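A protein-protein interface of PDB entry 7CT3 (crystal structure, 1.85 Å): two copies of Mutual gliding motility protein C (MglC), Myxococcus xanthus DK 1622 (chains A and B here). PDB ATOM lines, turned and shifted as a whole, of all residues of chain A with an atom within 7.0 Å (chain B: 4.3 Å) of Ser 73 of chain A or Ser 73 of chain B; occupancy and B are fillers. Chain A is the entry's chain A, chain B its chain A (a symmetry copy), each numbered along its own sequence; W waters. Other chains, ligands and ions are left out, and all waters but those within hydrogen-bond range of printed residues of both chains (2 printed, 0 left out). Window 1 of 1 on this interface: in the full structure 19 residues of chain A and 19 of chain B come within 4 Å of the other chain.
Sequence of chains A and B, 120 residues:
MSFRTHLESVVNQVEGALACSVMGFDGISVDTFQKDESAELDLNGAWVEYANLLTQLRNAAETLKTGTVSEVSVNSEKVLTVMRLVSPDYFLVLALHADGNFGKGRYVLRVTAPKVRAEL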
ATOM      1  N   LEU A  57      13.083 -21.582  -5.222  1.00  0.00           N
ATOM      2  CA  LEU A  57      13.592 -20.383  -4.500  1.00  0.00           C
ATOM      3  C   LEU A  57      15.115 -20.325  -4.649  1.00  0.00           C
ATOM      4  O   LEU A  57      15.630 -19.272  -5.045  1.00  0.00           O
ATOM      5  CB  LEU A  57      13.201 -20.435  -3.017  1.00  0.00           C
ATOM      6  CG  LEU A  57      11.729 -20.179  -2.710  1.00  0.00           C
ATOM      7  CD1 LEU A  57      11.436 -20.408  -1.237  1.00  0.00           C
ATOM      8  CD2 LEU A  57      11.329 -18.773  -3.111  1.00  0.00           C
ATOM      9  N   ALA A  60      16.220 -19.543  -8.352  1.00  0.00           N
ATOM     10  CA  ALA A  60      15.982 -18.120  -8.696  1.00  0.00           C
ATOM     11  C   ALA A  60      16.928 -17.222  -7.885  1.00  0.00           C
ATOM     12  O   ALA A  60      17.384 -16.193  -8.428  1.00  0.00           O
ATOM     13  CB  ALA A  60      14.534 -17.759  -8.471  1.00  0.00           C
ATOM     14  N   THR A  63      20.299 -15.579  -9.127  1.00  0.00           N
ATOM     15  CA  THR A  63      20.306 -14.301  -9.893  1.00  0.00           C
ATOM     16  C   THR A  63      20.770 -13.142  -8.996  1.00  0.00           C
ATOM     17  O   THR A  63      21.317 -12.166  -9.546  1.00  0.00           O
ATOM     18  CB  THR A  63      18.952 -14.020 -10.560  1.00  0.00           C
ATOM     19  OG1 THR A  63      17.961 -13.775  -9.563  1.00  0.00           O
ATOM     20  CG2 THR A  63      18.502 -15.143 -11.471  1.00  0.00           C
ATOM     21  N   VAL A  69      20.799  -7.306 -10.034  1.00  0.00           N
ATOM     22  CA  VAL A  69      19.655  -7.930  -9.306  1.00  0.00           C
ATOM     23  C   VAL A  69      19.839  -7.676  -7.805  1.00  0.00           C
ATOM     24  O   VAL A  69      20.888  -8.077  -7.254  1.00  0.00           O
ATOM     25  CB  VAL A  69      19.529  -9.429  -9.625  1.00  0.00           C
ATOM     26  CG1 VAL A  69      18.415 -10.078  -8.820  1.00  0.00           C
ATOM     27  CG2 VAL A  69      19.323  -9.671 -11.114  1.00  0.00           C
ATOM     28  N   GLU A  71      16.742  -7.961  -5.628  1.00  0.00           N
ATOM     29  CA  GLU A  71      15.571  -8.584  -4.956  1.00  0.00           C
ATOM     30  C   GLU A  71      14.887  -9.564  -5.918  1.00  0.00           C
ATOM     31  O   GLU A  71      14.715  -9.224  -7.103  1.00  0.00           O
ATOM     32  CB  GLU A  71      14.662  -7.452  -4.477  1.00  0.00           C
ATOM     33  CG  GLU A  71      13.391  -7.870  -3.771  1.00  0.00           C
ATOM     34  CD  GLU A  71      12.432  -6.691  -3.651  1.00  0.00           C
ATOM     35  OE1 GLU A  71      11.837  -6.316  -4.677  1.00  0.00           O
ATOM     36  OE2 GLU A  71      12.327  -6.110  -2.552  1.00  0.00           O
ATOM     37  N   VAL A  72      14.533 -10.751  -5.425  1.00  0.00           N
ATOM     38  CA  VAL A  72      13.855 -11.810  -6.225  1.00  0.00           C
ATOM     39  C   VAL A  72      12.658 -12.336  -5.430  1.00  0.00           C
ATOM     40  O   VAL A  72      12.779 -12.477  -4.200  1.00  0.00           O
ATOM     41  CB  VAL A  72      14.835 -12.938  -6.595  1.00  0.00           C
ATOM     42  CG1 VAL A  72      14.153 -14.030  -7.403  1.00  0.00           C
ATOM     43  CG2 VAL A  72      16.046 -12.394  -7.340  1.00  0.00           C
ATOM     44  N   SER A  73      11.551 -12.603  -6.123  1.00  0.00           N
ATOM     45  CA  SER A  73      10.324 -13.236  -5.570  1.00  0.00           C
ATOM     46  C   SER A  73       9.949 -14.445  -6.424  1.00  0.00           C
ATOM     47  O   SER A  73       9.944 -14.328  -7.665  1.00  0.00           O
ATOM     48  CB  SER A  73       9.184 -12.256  -5.500  1.00  0.00           C
ATOM     49  OG  SER A  73       9.469 -11.229  -4.569  1.00  0.00           O
ATOM     50  N   VAL A  74       9.655 -15.568  -5.775  1.00  0.00           N
ATOM     51  CA  VAL A  74       9.059 -16.765  -6.426  1.00  0.00           C
ATOM     52  C   VAL A  74       7.771 -17.069  -5.665  1.00  0.00           C
ATOM     53  O   VAL A  74       7.859 -17.406  -4.462  1.00  0.00           O
ATOM     54  CB  VAL A  74      10.042 -17.948  -6.443  1.00  0.00           C
ATOM     55  CG1 VAL A  74       9.413 -19.197  -7.032  1.00  0.00           C
ATOM     56  CG2 VAL A  74      11.321 -17.597  -7.191  1.00  0.00           C
ATOM     57  N   ASN A  75       6.628 -16.897  -6.329  1.00  0.00           N
ATOM     58  CA  ASN A  75       5.296 -16.866  -5.678  1.00  0.00           C
ATOM     59  C   ASN A  75       4.434 -18.016  -6.197  1.00  0.00           C
ATOM     60  O   ASN A  75       4.543 -18.375  -7.383  1.00  0.00           O
ATOM     61  CB  ASN A  75       4.598 -15.523  -5.896  1.00  0.00           C
ATOM     62  CG  ASN A  75       5.378 -14.351  -5.340  1.00  0.00           C
ATOM     63  OD1 ASN A  75       6.218 -14.516  -4.455  1.00  0.00           O
ATOM     64  ND2 ASN A  75       5.104 -13.160  -5.851  1.00  0.00           N
ATOM     65  N   LEU A  80       3.865 -16.024  -0.991  1.00  0.00           N
ATOM     66  CA  LEU A  80       4.748 -15.024  -1.634  1.00  0.00           C
ATOM     67  C   LEU A  80       6.105 -15.086  -0.938  1.00  0.00           C
ATOM     68  O   LEU A  80       6.136 -15.330   0.286  1.00  0.00           O
ATOM     69  CB  LEU A  80       4.127 -13.632  -1.507  1.00  0.00           C
ATOM     70  CG  LEU A  80       2.633 -13.541  -1.804  1.00  0.00           C
ATOM     71  CD1 LEU A  80       2.135 -12.122  -1.587  1.00  0.00           C
ATOM     72  CD2 LEU A  80       2.318 -14.007  -3.218  1.00  0.00           C
ATOM     73  N   THR A  81       7.184 -14.893  -1.691  1.00  0.00           N
ATOM     74  CA  THR A  81       8.557 -14.837  -1.138  1.00  0.00           C
ATOM     75  C   THR A  81       9.244 -13.564  -1.623  1.00  0.00           C
ATOM     76  O   THR A  81       8.887 -13.053  -2.708  1.00  0.00           O
ATOM     77  CB  THR A  81       9.373 -16.092  -1.463  1.00  0.00           C
ATOM     78  OG1 THR A  81       9.605 -16.137  -2.870  1.00  0.00           O
ATOM     79  CG2 THR A  81       8.694 -17.359  -0.989  1.00  0.00           C
ATOM     80  N   VAL A  82      10.168 -13.077  -0.803  1.00  0.00           N
ATOM     81  CA  VAL A  82      11.101 -11.961  -1.110  1.00  0.00           C
ATOM     82  C   VAL A  82      12.475 -12.423  -0.652  1.00  0.00           C
ATOM     83  O   VAL A  82      12.604 -12.901   0.474  1.00  0.00           O
ATOM     84  CB  VAL A  82      10.711 -10.660  -0.385  1.00  0.00           C
ATOM     85  CG1 VAL A  82      11.520  -9.488  -0.911  1.00  0.00           C
ATOM     86  CG2 VAL A  82       9.225 -10.380  -0.464  1.00  0.00           C
ATOM     87  N   MET A  83      13.475 -12.253  -1.521  1.00  0.00           N
ATOM     88  CA  MET A  83      14.828 -12.687  -1.226  1.00  0.00           C
ATOM     89  C   MET A  83      15.814 -11.575  -1.563  1.00  0.00           C
ATOM     90  O   MET A  83      15.643 -10.884  -2.567  1.00  0.00           O
ATOM     91  CB  MET A  83      15.163 -13.941  -2.034  1.00  0.00           C
ATOM     92  CG  MET A  83      14.337 -15.138  -1.665  1.00  0.00           C
ATOM     93  SD  MET A  83      14.682 -16.572  -2.927  1.00  0.00           S
ATOM     94  CE  MET A  83      13.460 -16.172  -4.407  1.00  0.00           C
ATOM     95  N   PHE A 102       2.463  -7.829   1.193  1.00  0.00           N
ATOM     96  CA  PHE A 102       3.652  -8.073   0.335  1.00  0.00           C
ATOM     97  C   PHE A 102       4.506  -6.800   0.266  1.00  0.00           C
ATOM     98  O   PHE A 102       5.740  -6.903   0.357  1.00  0.00           O
ATOM     99  CB  PHE A 102       3.219  -8.579  -1.043  1.00  0.00           C
ATOM    100  CG  PHE A 102       4.344  -9.065  -1.922  1.00  0.00           C
ATOM    101  CD1 PHE A 102       5.266  -9.990  -1.462  1.00  0.00           C
ATOM    102  CD2 PHE A 102       4.465  -8.617  -3.227  1.00  0.00           C
ATOM    103  CE1 PHE A 102       6.289 -10.445  -2.283  1.00  0.00           C
ATOM    104  CE2 PHE A 102       5.482  -9.076  -4.047  1.00  0.00           C
ATOM    105  CZ  PHE A 102       6.394  -9.989  -3.574  1.00  0.00           C
ATOM    106  N   ARG A 106       8.467  -6.515   1.450  1.00  0.00           N
ATOM    107  CA  ARG A 106       9.571  -6.038   0.574  1.00  0.00           C
ATOM    108  C   ARG A 106      10.337  -4.922   1.297  1.00  0.00           C
ATOM    109  O   ARG A 106      11.585  -4.971   1.327  1.00  0.00           O
ATOM    110  CB  ARG A 106       9.009  -5.578  -0.773  1.00  0.00           C
ATOM    111  CG  ARG A 106       8.438  -6.704  -1.621  1.00  0.00           C
ATOM    112  CD  ARG A 106       7.912  -6.233  -2.966  1.00  0.00           C
ATOM    113  NE  ARG A 106       8.948  -5.548  -3.728  1.00  0.00           N
ATOM    114  CZ  ARG A 106       8.942  -4.263  -4.072  1.00  0.00           C
ATOM    115  NH1 ARG A 106       7.922  -3.478  -3.766  1.00  0.00           N
ATOM    116  NH2 ARG A 106       9.964  -3.766  -4.746  1.00  0.00           N
ATOM    117  N   GLU B  71       4.158 -17.046 -10.287  1.00  0.00           N
ATOM    118  CA  GLU B  71       4.607 -15.646 -10.520  1.00  0.00           C
ATOM    119  C   GLU B  71       6.046 -15.478 -10.018  1.00  0.00           C
ATOM    120  O   GLU B  71       6.364 -15.974  -8.922  1.00  0.00           O
ATOM    121  CB  GLU B  71       3.600 -14.724  -9.833  1.00  0.00           C
ATOM    122  CG  GLU B  71       3.879 -13.240  -9.936  1.00  0.00           C
ATOM    123  CD  GLU B  71       3.015 -12.463  -8.947  1.00  0.00           C
ATOM    124  OE1 GLU B  71       3.315 -12.521  -7.741  1.00  0.00           O
ATOM    125  OE2 GLU B  71       2.012 -11.855  -9.372  1.00  0.00           O
ATOM    126  N   VAL B  72       6.892 -14.818 -10.810  1.00  0.00           N
ATOM    127  CA  VAL B  72       8.320 -14.564 -10.467  1.00  0.00           C
ATOM    128  C   VAL B  72       8.631 -13.087 -10.722  1.00  0.00           C
ATOM    129  O   VAL B  72       8.132 -12.541 -11.722  1.00  0.00           O
ATOM    130  CB  VAL B  72       9.255 -15.491 -11.261  1.00  0.00           C
ATOM    131  CG1 VAL B  72      10.716 -15.235 -10.928  1.00  0.00           C
ATOM    132  CG2 VAL B  72       8.901 -16.955 -11.039  1.00  0.00           C
ATOM    133  N   SER B  73       9.422 -12.481  -9.837  1.00  0.00           N
ATOM    134  CA  SER B  73       9.947 -11.095  -9.963  1.00  0.00           C
ATOM    135  C   SER B  73      11.466 -11.114  -9.805  1.00  0.00           C
ATOM    136  O   SER B  73      11.967 -11.762  -8.866  1.00  0.00           O
ATOM    137  CB  SER B  73       9.315 -10.174  -8.954  1.00  0.00           C
ATOM    138  OG  SER B  73       7.933 -10.025  -9.218  1.00  0.00           O
ATOM    139  N   VAL B  74      12.169 -10.430 -10.703  1.00  0.00           N
ATOM    140  CA  VAL B  74      13.625 -10.155 -10.576  1.00  0.00           C
ATOM    141  C   VAL B  74      13.784  -8.640 -10.650  1.00  0.00           C
ATOM    142  O   VAL B  74      13.471  -8.062 -11.716  1.00  0.00           O
ATOM    143  CB  VAL B  74      14.437 -10.898 -11.651  1.00  0.00           C
ATOM    144  CG1 VAL B  74      15.915 -10.560 -11.578  1.00  0.00           C
ATOM    145  CG2 VAL B  74      14.235 -12.406 -11.559  1.00  0.00           C
ATOM    146  N   ASN B  75      14.193  -8.025  -9.539  1.00  0.00           N
ATOM    147  CA  ASN B  75      14.128  -6.557  -9.341  1.00  0.00           C
ATOM    148  C   ASN B  75      15.537  -5.993  -9.154  1.00  0.00           C
ATOM    149  O   ASN B  75      16.392  -6.668  -8.554  1.00  0.00           O
ATOM    150  CB  ASN B  75      13.236  -6.193  -8.154  1.00  0.00           C
ATOM    151  CG  ASN B  75      11.808  -6.671  -8.316  1.00  0.00           C
ATOM    152  OD1 ASN B  75      11.348  -6.913  -9.432  1.00  0.00           O
ATOM    153  ND2 ASN B  75      11.099  -6.805  -7.207  1.00  0.00           N
ATOM    154  N   THR B  81      10.135  -6.270 -12.046  1.00  0.00           N
ATOM    155  CA  THR B  81       9.536  -7.157 -13.070  1.00  0.00           C
ATOM    156  C   THR B  81       8.545  -8.104 -12.400  1.00  0.00           C
ATOM    157  O   THR B  81       8.708  -8.407 -11.197  1.00  0.00           O
ATOM    158  CB  THR B  81      10.593  -7.912 -13.885  1.00  0.00           C
ATOM    159  OG1 THR B  81      11.261  -8.834 -13.025  1.00  0.00           O
ATOM    160  CG2 THR B  81      11.583  -6.978 -14.547  1.00  0.00           C
ATOM    161  N   VAL B  82       7.544  -8.508 -13.173  1.00  0.00           N
ATOM    162  CA  VAL B  82       6.550  -9.558 -12.828  1.00  0.00           C
ATOM    163  C   VAL B  82       6.437 -10.450 -14.054  1.00  0.00           C
ATOM    164  O   VAL B  82       6.274  -9.935 -15.159  1.00  0.00           O
ATOM    165  CB  VAL B  82       5.173  -8.964 -12.479  1.00  0.00           C
ATOM    166  CG1 VAL B  82       4.262 -10.026 -11.890  1.00  0.00           C
ATOM    167  CG2 VAL B  82       5.281  -7.763 -11.560  1.00  0.00           C
ATOM    168  N   PHE B 102       3.708  -1.373  -8.146  1.00  0.00           N
ATOM    169  CA  PHE B 102       4.084  -2.808  -8.240  1.00  0.00           C
ATOM    170  C   PHE B 102       2.857  -3.680  -7.944  1.00  0.00           C
ATOM    171  O   PHE B 102       2.646  -4.674  -8.657  1.00  0.00           O
ATOM    172  CB  PHE B 102       5.270  -3.109  -7.321  1.00  0.00           C
ATOM    173  CG  PHE B 102       5.874  -4.480  -7.493  1.00  0.00           C
ATOM    174  CD1 PHE B 102       6.249  -4.945  -8.743  1.00  0.00           C
ATOM    175  CD2 PHE B 102       6.098  -5.296  -6.399  1.00  0.00           C
ATOM    176  CE1 PHE B 102       6.821  -6.202  -8.892  1.00  0.00           C
ATOM    177  CE2 PHE B 102       6.673  -6.547  -6.547  1.00  0.00           C
ATOM    178  CZ  PHE B 102       7.034  -6.999  -7.795  1.00  0.00           C
HETATM  179  O   HOH W   1       5.884 -10.680  -7.430  1.00  0.00           O
HETATM  180  O   HOH W   2       9.588  -8.502  -5.184  1.00  0.00           O
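The side-chain carboxylate (OE1) of Glu 71 of chain A is in hydrogen-bond range of the side-chain amide nitrogen (ND2) of Asn 75 of chain B (2.7 Å). N of Ser 73 of chain B lies within hydrogen-bond range of O of Ser 73 of chain A (2.9 Å). ND2 of Asn 75 of chain A lies within hydrogen-bond range of OE1 of Glu 71 of chain B (2.7 Å).
The side-chain carboxylate (OE1) of Glu 71 of chain A is in salt-bridge range of the guanidinium group (NE) of Arg 106 of chain A. The backbone NH of Met 83 of chain A lies within hydrogen-bond range of the backbone carbonyl oxygen of Val 72 of chain A (2.8 Å). The side-chain hydroxyl (OG) of Ser 73 of chain A sits at hydrogen-bond distance from the backbone carbonyl oxygen (O) of Thr 81 of chain A, at 2.7 Å. N of Thr 81 of chain A is in hydrogen-bond range of OD1 of Asn 75 of chain A (3.0 Å). The backbone carbonyl oxygen (O) of Thr 81 of chain B lies within hydrogen-bond range of the side-chain hydroxyl (OG) of Ser 73 of chain B, 2.7 Å away. The backbone carbonyl oxygen (O) of Val 74 of chain B is in hydrogen-bond range of the side-chain hydroxyl (OG1) of Thr 81 of chain B, 2.7 Å away.
Among the printed residues, merely in contact across the chains: Val 72 of chain A with Ser 73 of chain B (3.2 Å), Ser 73 of chain A with Val 72 of chain B (3.2 Å), Val 69 of chain A with Val 74 of chain B (3.6 Å), Val 69 of chain A with Asn 75 of chain B (3.6 Å), Arg 106 of chain A with Phe 102 of chain B (3.7 Å), Val 74 of chain A with Glu 71 of chain B (3.7 Å), Glu 71 of chain A with Val 74 of chain B (3.7 Å) and Phe 102 of chain A with Phe 102 of chain B (3.8 Å).
Of the printed residues of chain B, Ser 73 of chain A touches Val 72 (3.2 Å) and Ser 73 (2.9 Å). Ser 73 of chain B touches just these residues of chain A: Val 72 (3.2 Å) and Ser 73 (2.9 Å). Printed residues of chain B within 4 Å of Asn 75 of chain A: Glu 71 (2.7 Å). Of the printed residues of chain A, Val 74 of chain B touches Val 69 and Glu 71. Of the printed residues of chain A, Glu 71 of chain B touches Val 74 (3.7 Å) and Asn 75 (2.7 Å). Printed residues of chain A within 4 Å of Val 72 of chain B: Ser 73 (3.2 Å). The nearest residue of chain B that does not touch Ser 73 of chain A is Glu 71 of chain B (4.1 Å). The nearest residue of chain A that does not touch Ser 73 of chain B is Glu 71 of chain A (4.1 Å).
Of the 8 printed residues of chain B, 6 touch a printed residue of chain A. Printed residues of chain B that touch a printed residue of chain A: Glu 71, Val 72, Ser 73, Val 74, Asn 75 and Phe 102. Hydrophobic or aromatic side chains of chain B within 4 Å of the printed part of chain A: Val 72, Val 74 and Phe 102. Among the printed residues, no Asp or Glu carboxylate lies within 4 Å of a Lys or Arg side-chain nitrogen of the other chain.
Glu 71 of chain A touches Val 74 of chain B, and with the chains exchanged Val 74 of chain A touches Glu 71 of chain B. Glu 71 of chain A touches Asn 75 of chain B, and with the chains exchanged Asn 75 of chain A touches Glu 71 of chain B. Val 72 of chain A touches Ser 73 of chain B, and with the chains exchanged Ser 73 of chain A touches Val 72 of chain B. Phe 102 of chain A touches its own counterpart, Phe 102 of chain B.
Water W1 lies within hydrogen-bond range of the side-chain hydroxyl of Ser 73 of chain B, the side-chain amide nitrogen of Asn 75 of chain A and the side-chain carboxylate of Glu 71 of chain B. Water W2 lies within hydrogen-bond range of the side-chain hydroxyl (OG) of Ser 73 of chain A, the side-chain amide nitrogen (ND2) of Asn 75 of chain B, the side-chain carboxylate (OE1) of Glu 71 of chain A and the guanidinium group (NE) of Arg 106 of chain A.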
